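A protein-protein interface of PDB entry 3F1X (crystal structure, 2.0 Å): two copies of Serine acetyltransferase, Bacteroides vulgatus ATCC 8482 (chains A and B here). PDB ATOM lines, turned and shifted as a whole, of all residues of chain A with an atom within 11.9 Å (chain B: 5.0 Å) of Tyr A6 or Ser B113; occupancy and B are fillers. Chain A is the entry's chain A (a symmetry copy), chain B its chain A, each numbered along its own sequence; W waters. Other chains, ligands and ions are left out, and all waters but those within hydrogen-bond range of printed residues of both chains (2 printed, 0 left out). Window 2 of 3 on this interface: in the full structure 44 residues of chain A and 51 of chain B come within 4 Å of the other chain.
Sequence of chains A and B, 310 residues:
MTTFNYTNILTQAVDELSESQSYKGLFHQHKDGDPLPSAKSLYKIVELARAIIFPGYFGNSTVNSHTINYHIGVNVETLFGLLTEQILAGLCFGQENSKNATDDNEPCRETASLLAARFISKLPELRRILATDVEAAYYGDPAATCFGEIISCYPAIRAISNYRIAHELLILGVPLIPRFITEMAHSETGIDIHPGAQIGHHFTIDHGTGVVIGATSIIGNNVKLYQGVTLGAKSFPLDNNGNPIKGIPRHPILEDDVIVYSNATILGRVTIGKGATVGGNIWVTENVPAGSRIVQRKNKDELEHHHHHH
Tyr A6 touches three residues of chain B.
No residue of chain A comes within 4 Å of Glu B110.
No residue of chain A comes within 4 Å of Thr B111.
No residue of chain A comes within 4 Å of Ala B112.
No residue of chain A comes within 4 Å of Leu B115.
Printed residues of chain A within 4 Å of Ala B117: Tyr A6 and Ile A9.
Printed residues of chain A within 4 Å of Phe B80: Tyr A6 and Leu A10.
Of the printed residues of chain B, Asn A5 touches Leu B114 (3.5 Å).
Of the printed residues of chain B, Ile A9 touches Leu B114 (3.7 Å) and Ala B117 (3.4 Å).
Of the printed residues of chain B, Leu A10 touches Phe B80 (3.8 Å).
Thr A3 touches none of the printed residues of chain B.
The nearest residue of chain B that does not touch Tyr A6 is Leu B114 (4.5 Å).
The nearest residue of chain A that does not touch Ser B113 is Asn A5 (5.2 Å).
The nearest printed residue of chain B that does not touch Ile A9 is Ala B116 (6.7 Å).
No position is printed for both chains.
Among the printed residues, merely in contact across the chains: Ile A9 with Ala B117, Asn A5 with Leu B114, Tyr A6 with Phe B80, Tyr A6 with Ala B117, Ile A9 with Leu B114, Leu A10 with Phe B80 and Tyr A6 with Ser B113.
Printed residues of chain A that touch a printed residue of chain B: Asn A5, Tyr A6, Ile A9 and Leu A10.
Of the 11 printed residues of chain B, 4 touch a printed residue of chain A.
Hydrophobic or aromatic side chains of chain B within 4 Å of the printed part of chain A: Phe B80, Leu B114 and Ala B117.
Among the printed residues, 7 pairs touch across the chains.
Among the printed residues, no Asp or Glu carboxylate lies within 4 Å of a Lys or Arg side-chain nitrogen of the other chain.
O of Arg B109 lies within hydrogen-bond range of OG of Ser B113.
The backbone carbonyl oxygen (O) of Phe B80 lies within hydrogen-bond range of the side-chain hydroxyl (OG1) of Thr B84 (2.7 Å).
O of Glu B110 lies within hydrogen-bond range of OG of Ser B113 (2.9 Å).
Water W1 lies within hydrogen-bond range of O of Glu B110 (2.7 Å) and ND2 of Asn A5 (3.4 Å).
Water W2 lies within hydrogen-bond range of OG of Ser B113 (2.8 Å), O of Glu B110 (2.8 Å) and OD1 of Asn A5 (3.0 Å).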
ATOM      1  N   THR A   2      -7.935  25.114 -17.668  1.00  0.00           N
ATOM      2  CA  THR A   2      -7.005  26.093 -18.297  1.00  0.00           C
ATOM      3  C   THR A   2      -6.257  25.462 -19.469  1.00  0.00           C
ATOM      4  O   THR A   2      -6.203  24.234 -19.603  1.00  0.00           O
ATOM      5  CB  THR A   2      -5.974  26.615 -17.278  1.00  0.00           C
ATOM      6  OG1 THR A   2      -5.329  25.509 -16.639  1.00  0.00           O
ATOM      7  CG2 THR A   2      -6.651  27.475 -16.226  1.00  0.00           C
ATOM      8  N   THR A   3      -5.674  26.311 -20.308  1.00  0.00           N
ATOM      9  CA  THR A   3      -4.931  25.846 -21.470  1.00  0.00           C
ATOM     10  C   THR A   3      -3.432  26.097 -21.332  1.00  0.00           C
ATOM     11  O   THR A   3      -2.985  27.245 -21.321  1.00  0.00           O
ATOM     12  CB  THR A   3      -5.418  26.543 -22.768  1.00  0.00           C
ATOM     13  OG1 THR A   3      -6.802  26.243 -22.990  1.00  0.00           O
ATOM     14  CG2 THR A   3      -4.603  26.068 -23.975  1.00  0.00           C
ATOM     15  N   PHE A   4      -2.664  25.016 -21.219  1.00  0.00           N
ATOM     16  CA  PHE A   4      -1.205  25.113 -21.122  1.00  0.00           C
ATOM     17  C   PHE A   4      -0.662  24.922 -22.539  1.00  0.00           C
ATOM     18  O   PHE A   4      -1.423  24.662 -23.467  1.00  0.00           O
ATOM     19  CB  PHE A   4      -0.653  24.010 -20.223  1.00  0.00           C
ATOM     20  CG  PHE A   4      -1.151  24.072 -18.815  1.00  0.00           C
ATOM     21  CD1 PHE A   4      -0.726  25.086 -17.952  1.00  0.00           C
ATOM     22  CD2 PHE A   4      -2.047  23.114 -18.342  1.00  0.00           C
ATOM     23  CE1 PHE A   4      -1.188  25.141 -16.634  1.00  0.00           C
ATOM     24  CE2 PHE A   4      -2.512  23.164 -17.027  1.00  0.00           C
ATOM     25  CZ  PHE A   4      -2.081  24.179 -16.169  1.00  0.00           C
ATOM     26  N   ASN A   5       0.648  25.028 -22.708  1.00  0.00           N
ATOM     27  CA  ASN A   5       1.229  24.864 -24.032  1.00  0.00           C
ATOM     28  C   ASN A   5       1.133  23.422 -24.523  1.00  0.00           C
ATOM     29  O   ASN A   5       1.147  23.175 -25.725  1.00  0.00           O
ATOM     30  CB  ASN A   5       2.687  25.341 -24.032  1.00  0.00           C
ATOM     31  CG  ASN A   5       3.572  24.515 -23.122  1.00  0.00           C
ATOM     32  OD1 ASN A   5       3.092  23.858 -22.195  1.00  0.00           O
ATOM     33  ND2 ASN A   5       4.876  24.556 -23.369  1.00  0.00           N
ATOM     34  N   TYR A   6       1.015  22.473 -23.599  1.00  0.00           N
ATOM     35  CA  TYR A   6       0.915  21.062 -23.970  1.00  0.00           C
ATOM     36  C   TYR A   6      -0.527  20.561 -24.093  1.00  0.00           C
ATOM     37  O   TYR A   6      -0.773  19.483 -24.629  1.00  0.00           O
ATOM     38  CB  TYR A   6       1.682  20.204 -22.955  1.00  0.00           C
ATOM     39  CG  TYR A   6       1.268  20.404 -21.513  1.00  0.00           C
ATOM     40  CD1 TYR A   6       0.059  19.909 -21.034  1.00  0.00           C
ATOM     41  CD2 TYR A   6       2.085  21.109 -20.633  1.00  0.00           C
ATOM     42  CE1 TYR A   6      -0.331  20.114 -19.704  1.00  0.00           C
ATOM     43  CE2 TYR A   6       1.708  21.321 -19.307  1.00  0.00           C
ATOM     44  CZ  TYR A   6       0.503  20.822 -18.849  1.00  0.00           C
ATOM     45  OH  TYR A   6       0.142  21.033 -17.537  1.00  0.00           O
ATOM     46  N   THR A   7      -1.478  21.356 -23.617  1.00  0.00           N
ATOM     47  CA  THR A   7      -2.885  20.980 -23.648  1.00  0.00           C
ATOM     48  C   THR A   7      -3.442  20.556 -25.002  1.00  0.00           C
ATOM     49  O   THR A   7      -3.989  19.460 -25.134  1.00  0.00           O
ATOM     50  CB  THR A   7      -3.761  22.119 -23.109  1.00  0.00           C
ATOM     51  OG1 THR A   7      -3.333  22.447 -21.786  1.00  0.00           O
ATOM     52  CG2 THR A   7      -5.223  21.708 -23.084  1.00  0.00           C
ATOM     53  N   ASN A   8      -3.320  21.420 -26.005  1.00  0.00           N
ATOM     54  CA  ASN A   8      -3.837  21.105 -27.329  1.00  0.00           C
ATOM     55  C   ASN A   8      -3.049  19.997 -28.017  1.00  0.00           C
ATOM     56  O   ASN A   8      -3.571  19.316 -28.901  1.00  0.00           O
ATOM     57  CB  ASN A   8      -3.878  22.368 -28.200  1.00  0.00           C
ATOM     58  CG  ASN A   8      -4.877  23.399 -27.681  1.00  0.00           C
ATOM     59  OD1 ASN A   8      -5.758  23.073 -26.876  1.00  0.00           O
ATOM     60  ND2 ASN A   8      -4.757  24.639 -28.145  1.00  0.00           N
ATOM     61  N   ILE A   9      -1.800  19.802 -27.607  1.00  0.00           N
ATOM     62  CA  ILE A   9      -0.980  18.747 -28.186  1.00  0.00           C
ATOM     63  C   ILE A   9      -1.568  17.409 -27.752  1.00  0.00           C
ATOM     64  O   ILE A   9      -1.713  16.495 -28.557  1.00  0.00           O
ATOM     65  CB  ILE A   9       0.483  18.848 -27.708  1.00  0.00           C
ATOM     66  CG1 ILE A   9       1.114  20.120 -28.258  1.00  0.00           C
ATOM     67  CG2 ILE A   9       1.285  17.633 -28.191  1.00  0.00           C
ATOM     68  CD1 ILE A   9       2.441  20.461 -27.628  1.00  0.00           C
ATOM     69  N   LEU A  10      -1.925  17.319 -26.474  1.00  0.00           N
ATOM     70  CA  LEU A  10      -2.507  16.101 -25.922  1.00  0.00           C
ATOM     71  C   LEU A  10      -3.881  15.787 -26.510  1.00  0.00           C
ATOM     72  O   LEU A  10      -4.166  14.641 -26.864  1.00  0.00           O
ATOM     73  CB  LEU A  10      -2.620  16.209 -24.398  1.00  0.00           C
ATOM     74  CG  LEU A  10      -1.306  16.317 -23.627  1.00  0.00           C
ATOM     75  CD1 LEU A  10      -1.591  16.415 -22.133  1.00  0.00           C
ATOM     76  CD2 LEU A  10      -0.435  15.091 -23.928  1.00  0.00           C
ATOM     77  N   THR A  11      -4.739  16.798 -26.614  1.00  0.00           N
ATOM     78  CA  THR A  11      -6.077  16.572 -27.152  1.00  0.00           C
ATOM     79  C   THR A  11      -6.016  16.151 -28.616  1.00  0.00           C
ATOM     80  O   THR A  11      -6.749  15.257 -29.049  1.00  0.00           O
ATOM     81  CB  THR A  11      -6.976  17.827 -26.987  1.00  0.00           C
ATOM     82  OG1 THR A  11      -6.299  18.986 -27.495  1.00  0.00           O
ATOM     83  CG2 THR A  11      -7.308  18.050 -25.515  1.00  0.00           C
ATOM     84  N   GLN A  12      -5.134  16.776 -29.382  1.00  0.00           N
ATOM     85  CA  GLN A  12      -5.015  16.411 -30.786  1.00  0.00           C
ATOM     86  C   GLN A  12      -4.495  14.979 -30.909  1.00  0.00           C
ATOM     87  O   GLN A  12      -4.916  14.234 -31.798  1.00  0.00           O
ATOM     88  CB  GLN A  12      -4.082  17.382 -31.503  1.00  0.00           C
ATOM     89  CG  GLN A  12      -3.938  17.109 -32.998  1.00  0.00           C
ATOM     90  CD  GLN A  12      -5.274  17.042 -33.726  1.00  0.00           C
ATOM     91  OE1 GLN A  12      -6.133  17.913 -33.564  1.00  0.00           O
ATOM     92  NE2 GLN A  12      -5.450  16.011 -34.543  1.00  0.00           N
ATOM     93  N   ALA A  13      -3.592  14.585 -30.014  1.00  0.00           N
ATOM     94  CA  ALA A  13      -3.048  13.231 -30.053  1.00  0.00           C
ATOM     95  C   ALA A  13      -4.170  12.226 -29.818  1.00  0.00           C
ATOM     96  O   ALA A  13      -4.286  11.231 -30.530  1.00  0.00           O
ATOM     97  CB  ALA A  13      -1.956  13.059 -28.995  1.00  0.00           C
ATOM     98  N   VAL A  14      -5.000  12.501 -28.819  1.00  0.00           N
ATOM     99  CA  VAL A  14      -6.107  11.616 -28.501  1.00  0.00           C
ATOM    100  C   VAL A  14      -7.071  11.472 -29.681  1.00  0.00           C
ATOM    101  O   VAL A  14      -7.510  10.360 -29.994  1.00  0.00           O
ATOM    102  CB  VAL A  14      -6.879  12.117 -27.264  1.00  0.00           C
ATOM    103  CG1 VAL A  14      -8.165  11.306 -27.079  1.00  0.00           C
ATOM    104  CG2 VAL A  14      -5.992  12.001 -26.027  1.00  0.00           C
ATOM    105  N   ASP A  15      -7.392  12.580 -30.341  1.00  0.00           N
ATOM    106  CA  ASP A  15      -8.308  12.533 -31.483  1.00  0.00           C
ATOM    107  C   ASP A  15      -7.795  11.612 -32.585  1.00  0.00           C
ATOM    108  O   ASP A  15      -8.553  10.814 -33.131  1.00  0.00           O
ATOM    109  CB  ASP A  15      -8.533  13.937 -32.063  1.00  0.00           C
ATOM    110  CG  ASP A  15      -9.163  14.887 -31.059  1.00  0.00           C
ATOM    111  OD1 ASP A  15      -9.901  14.406 -30.171  1.00  0.00           O
ATOM    112  OD2 ASP A  15      -8.935  16.111 -31.169  1.00  0.00           O
ATOM    113  N   GLU A  16      -6.508  11.726 -32.898  1.00  0.00           N
ATOM    114  CA  GLU A  16      -5.878  10.909 -33.933  1.00  0.00           C
ATOM    115  C   GLU A  16      -5.829   9.440 -33.557  1.00  0.00           C
ATOM    116  O   GLU A  16      -6.032   8.564 -34.392  1.00  0.00           O
ATOM    117  CB  GLU A  16      -4.449  11.377 -34.187  1.00  0.00           C
ATOM    118  CG  GLU A  16      -4.316  12.675 -34.933  1.00  0.00           C
ATOM    119  CD  GLU A  16      -2.868  12.967 -35.287  1.00  0.00           C
ATOM    120  OE1 GLU A  16      -2.228  12.118 -35.951  1.00  0.00           O
ATOM    121  OE2 GLU A  16      -2.365  14.043 -34.902  1.00  0.00           O
ATOM    122  N   PHE B  80       1.009  10.807 -19.638  1.00  0.00           N
ATOM    123  CA  PHE B  80       1.559  12.148 -19.620  1.00  0.00           C
ATOM    124  C   PHE B  80       2.153  12.523 -18.269  1.00  0.00           C
ATOM    125  O   PHE B  80       3.253  13.068 -18.203  1.00  0.00           O
ATOM    126  CB  PHE B  80       0.487  13.164 -19.984  1.00  0.00           C
ATOM    127  CG  PHE B  80       0.962  14.579 -19.918  1.00  0.00           C
ATOM    128  CD1 PHE B  80       2.019  15.006 -20.710  1.00  0.00           C
ATOM    129  CD2 PHE B  80       0.360  15.491 -19.057  1.00  0.00           C
ATOM    130  CE1 PHE B  80       2.479  16.322 -20.647  1.00  0.00           C
ATOM    131  CE2 PHE B  80       0.812  16.812 -18.985  1.00  0.00           C
ATOM    132  CZ  PHE B  80       1.872  17.224 -19.784  1.00  0.00           C
ATOM    133  N   THR B  84       6.214  12.759 -17.755  1.00  0.00           N
ATOM    134  CA  THR B  84       6.779  14.073 -17.446  1.00  0.00           C
ATOM    135  C   THR B  84       7.820  13.922 -16.337  1.00  0.00           C
ATOM    136  O   THR B  84       8.938  14.418 -16.444  1.00  0.00           O
ATOM    137  CB  THR B  84       5.679  15.063 -16.977  1.00  0.00           C
ATOM    138  OG1 THR B  84       4.761  15.312 -18.053  1.00  0.00           O
ATOM    139  CG2 THR B  84       6.297  16.379 -16.529  1.00  0.00           C
ATOM    140  N   ARG B 109      10.095  21.147 -14.632  1.00  0.00           N
ATOM    141  CA  ARG B 109       9.047  20.265 -15.124  1.00  0.00           C
ATOM    142  C   ARG B 109       8.450  20.809 -16.418  1.00  0.00           C
ATOM    143  O   ARG B 109       7.981  20.055 -17.267  1.00  0.00           O
ATOM    144  CB  ARG B 109       7.956  20.132 -14.065  1.00  0.00           C
ATOM    145  CG  ARG B 109       6.804  19.221 -14.446  1.00  0.00           C
ATOM    146  CD  ARG B 109       5.870  19.080 -13.266  1.00  0.00           C
ATOM    147  NE  ARG B 109       6.614  18.685 -12.073  1.00  0.00           N
ATOM    148  CZ  ARG B 109       7.122  17.474 -11.874  1.00  0.00           C
ATOM    149  NH1 ARG B 109       6.961  16.525 -12.790  1.00  0.00           N
ATOM    150  NH2 ARG B 109       7.801  17.218 -10.766  1.00  0.00           N
ATOM    151  N   GLU B 110       8.469  22.131 -16.547  1.00  0.00           N
ATOM    152  CA  GLU B 110       7.944  22.813 -17.721  1.00  0.00           C
ATOM    153  C   GLU B 110       8.569  22.242 -18.993  1.00  0.00           C
ATOM    154  O   GLU B 110       7.878  21.976 -19.976  1.00  0.00           O
ATOM    155  CB  GLU B 110       8.254  24.306 -17.603  1.00  0.00           C
ATOM    156  CG  GLU B 110       7.937  25.137 -18.829  1.00  0.00           C
ATOM    157  CD  GLU B 110       8.449  26.563 -18.695  1.00  0.00           C
ATOM    158  OE1 GLU B 110       8.388  27.317 -19.689  1.00  0.00           O
ATOM    159  OE2 GLU B 110       8.912  26.931 -17.591  1.00  0.00           O
ATOM    160  N   THR B 111       9.882  22.056 -18.963  1.00  0.00           N
ATOM    161  CA  THR B 111      10.603  21.515 -20.103  1.00  0.00           C
ATOM    162  C   THR B 111      10.229  20.048 -20.315  1.00  0.00           C
ATOM    163  O   THR B 111       9.998  19.612 -21.441  1.00  0.00           O
ATOM    164  CB  THR B 111      12.125  21.592 -19.884  1.00  0.00           C
ATOM    165  OG1 THR B 111      12.487  22.927 -19.513  1.00  0.00           O
ATOM    166  CG2 THR B 111      12.871  21.203 -21.149  1.00  0.00           C
ATOM    167  N   ALA B 112      10.171  19.296 -19.221  1.00  0.00           N
ATOM    168  CA  ALA B 112       9.844  17.878 -19.275  1.00  0.00           C
ATOM    169  C   ALA B 112       8.411  17.618 -19.718  1.00  0.00           C
ATOM    170  O   ALA B 112       8.152  16.660 -20.438  1.00  0.00           O
ATOM    171  CB  ALA B 112      10.089  17.234 -17.909  1.00  0.00           C
ATOM    172  N   SER B 113       7.478  18.465 -19.298  1.00  0.00           N
ATOM    173  CA  SER B 113       6.083  18.251 -19.671  1.00  0.00           C
ATOM    174  C   SER B 113       5.842  18.440 -21.169  1.00  0.00           C
ATOM    175  O   SER B 113       5.054  17.713 -21.769  1.00  0.00           O
ATOM    176  CB  SER B 113       5.165  19.167 -18.849  1.00  0.00           C
ATOM    177  OG  SER B 113       5.496  20.527 -19.036  1.00  0.00           O
ATOM    178  N   LEU B 114       6.530  19.404 -21.780  1.00  0.00           N
ATOM    179  CA  LEU B 114       6.364  19.637 -23.210  1.00  0.00           C
ATOM    180  C   LEU B 114       6.984  18.478 -24.007  1.00  0.00           C
ATOM    181  O   LEU B 114       6.420  18.023 -25.003  1.00  0.00           O
ATOM    182  CB  LEU B 114       6.998  20.972 -23.610  1.00  0.00           C
ATOM    183  CG  LEU B 114       6.759  21.453 -25.047  1.00  0.00           C
ATOM    184  CD1 LEU B 114       5.271  21.403 -25.374  1.00  0.00           C
ATOM    185  CD2 LEU B 114       7.293  22.869 -25.202  1.00  0.00           C
ATOM    186  N   LEU B 115       8.140  17.994 -23.562  1.00  0.00           N
ATOM    187  CA  LEU B 115       8.781  16.872 -24.238  1.00  0.00           C
ATOM    188  C   LEU B 115       7.859  15.660 -24.136  1.00  0.00           C
ATOM    189  O   LEU B 115       7.683  14.916 -25.100  1.00  0.00           O
ATOM    190  CB  LEU B 115      10.141  16.553 -23.598  1.00  0.00           C
ATOM    191  CG  LEU B 115      11.298  17.539 -23.796  1.00  0.00           C
ATOM    192  CD1 LEU B 115      12.537  17.029 -23.074  1.00  0.00           C
ATOM    193  CD2 LEU B 115      11.596  17.701 -25.280  1.00  0.00           C
ATOM    194  N   ALA B 116       7.256  15.467 -22.967  1.00  0.00           N
ATOM    195  CA  ALA B 116       6.349  14.340 -22.767  1.00  0.00           C
ATOM    196  C   ALA B 116       5.159  14.456 -23.711  1.00  0.00           C
ATOM    197  O   ALA B 116       4.721  13.463 -24.288  1.00  0.00           O
ATOM    198  CB  ALA B 116       5.873  14.293 -21.318  1.00  0.00           C
ATOM    199  N   ALA B 117       4.643  15.673 -23.876  1.00  0.00           N
ATOM    200  CA  ALA B 117       3.512  15.884 -24.772  1.00  0.00           C
ATOM    201  C   ALA B 117       3.957  15.653 -26.224  1.00  0.00           C
ATOM    202  O   ALA B 117       3.215  15.078 -27.028  1.00  0.00           O
ATOM    203  CB  ALA B 117       2.955  17.297 -24.595  1.00  0.00           C
HETATM  204  O   HOH W   1       7.775  24.082 -21.725  1.00  0.00           O
HETATM  205  O   HOH W   2       5.281  22.970 -20.413  1.00  0.00           O
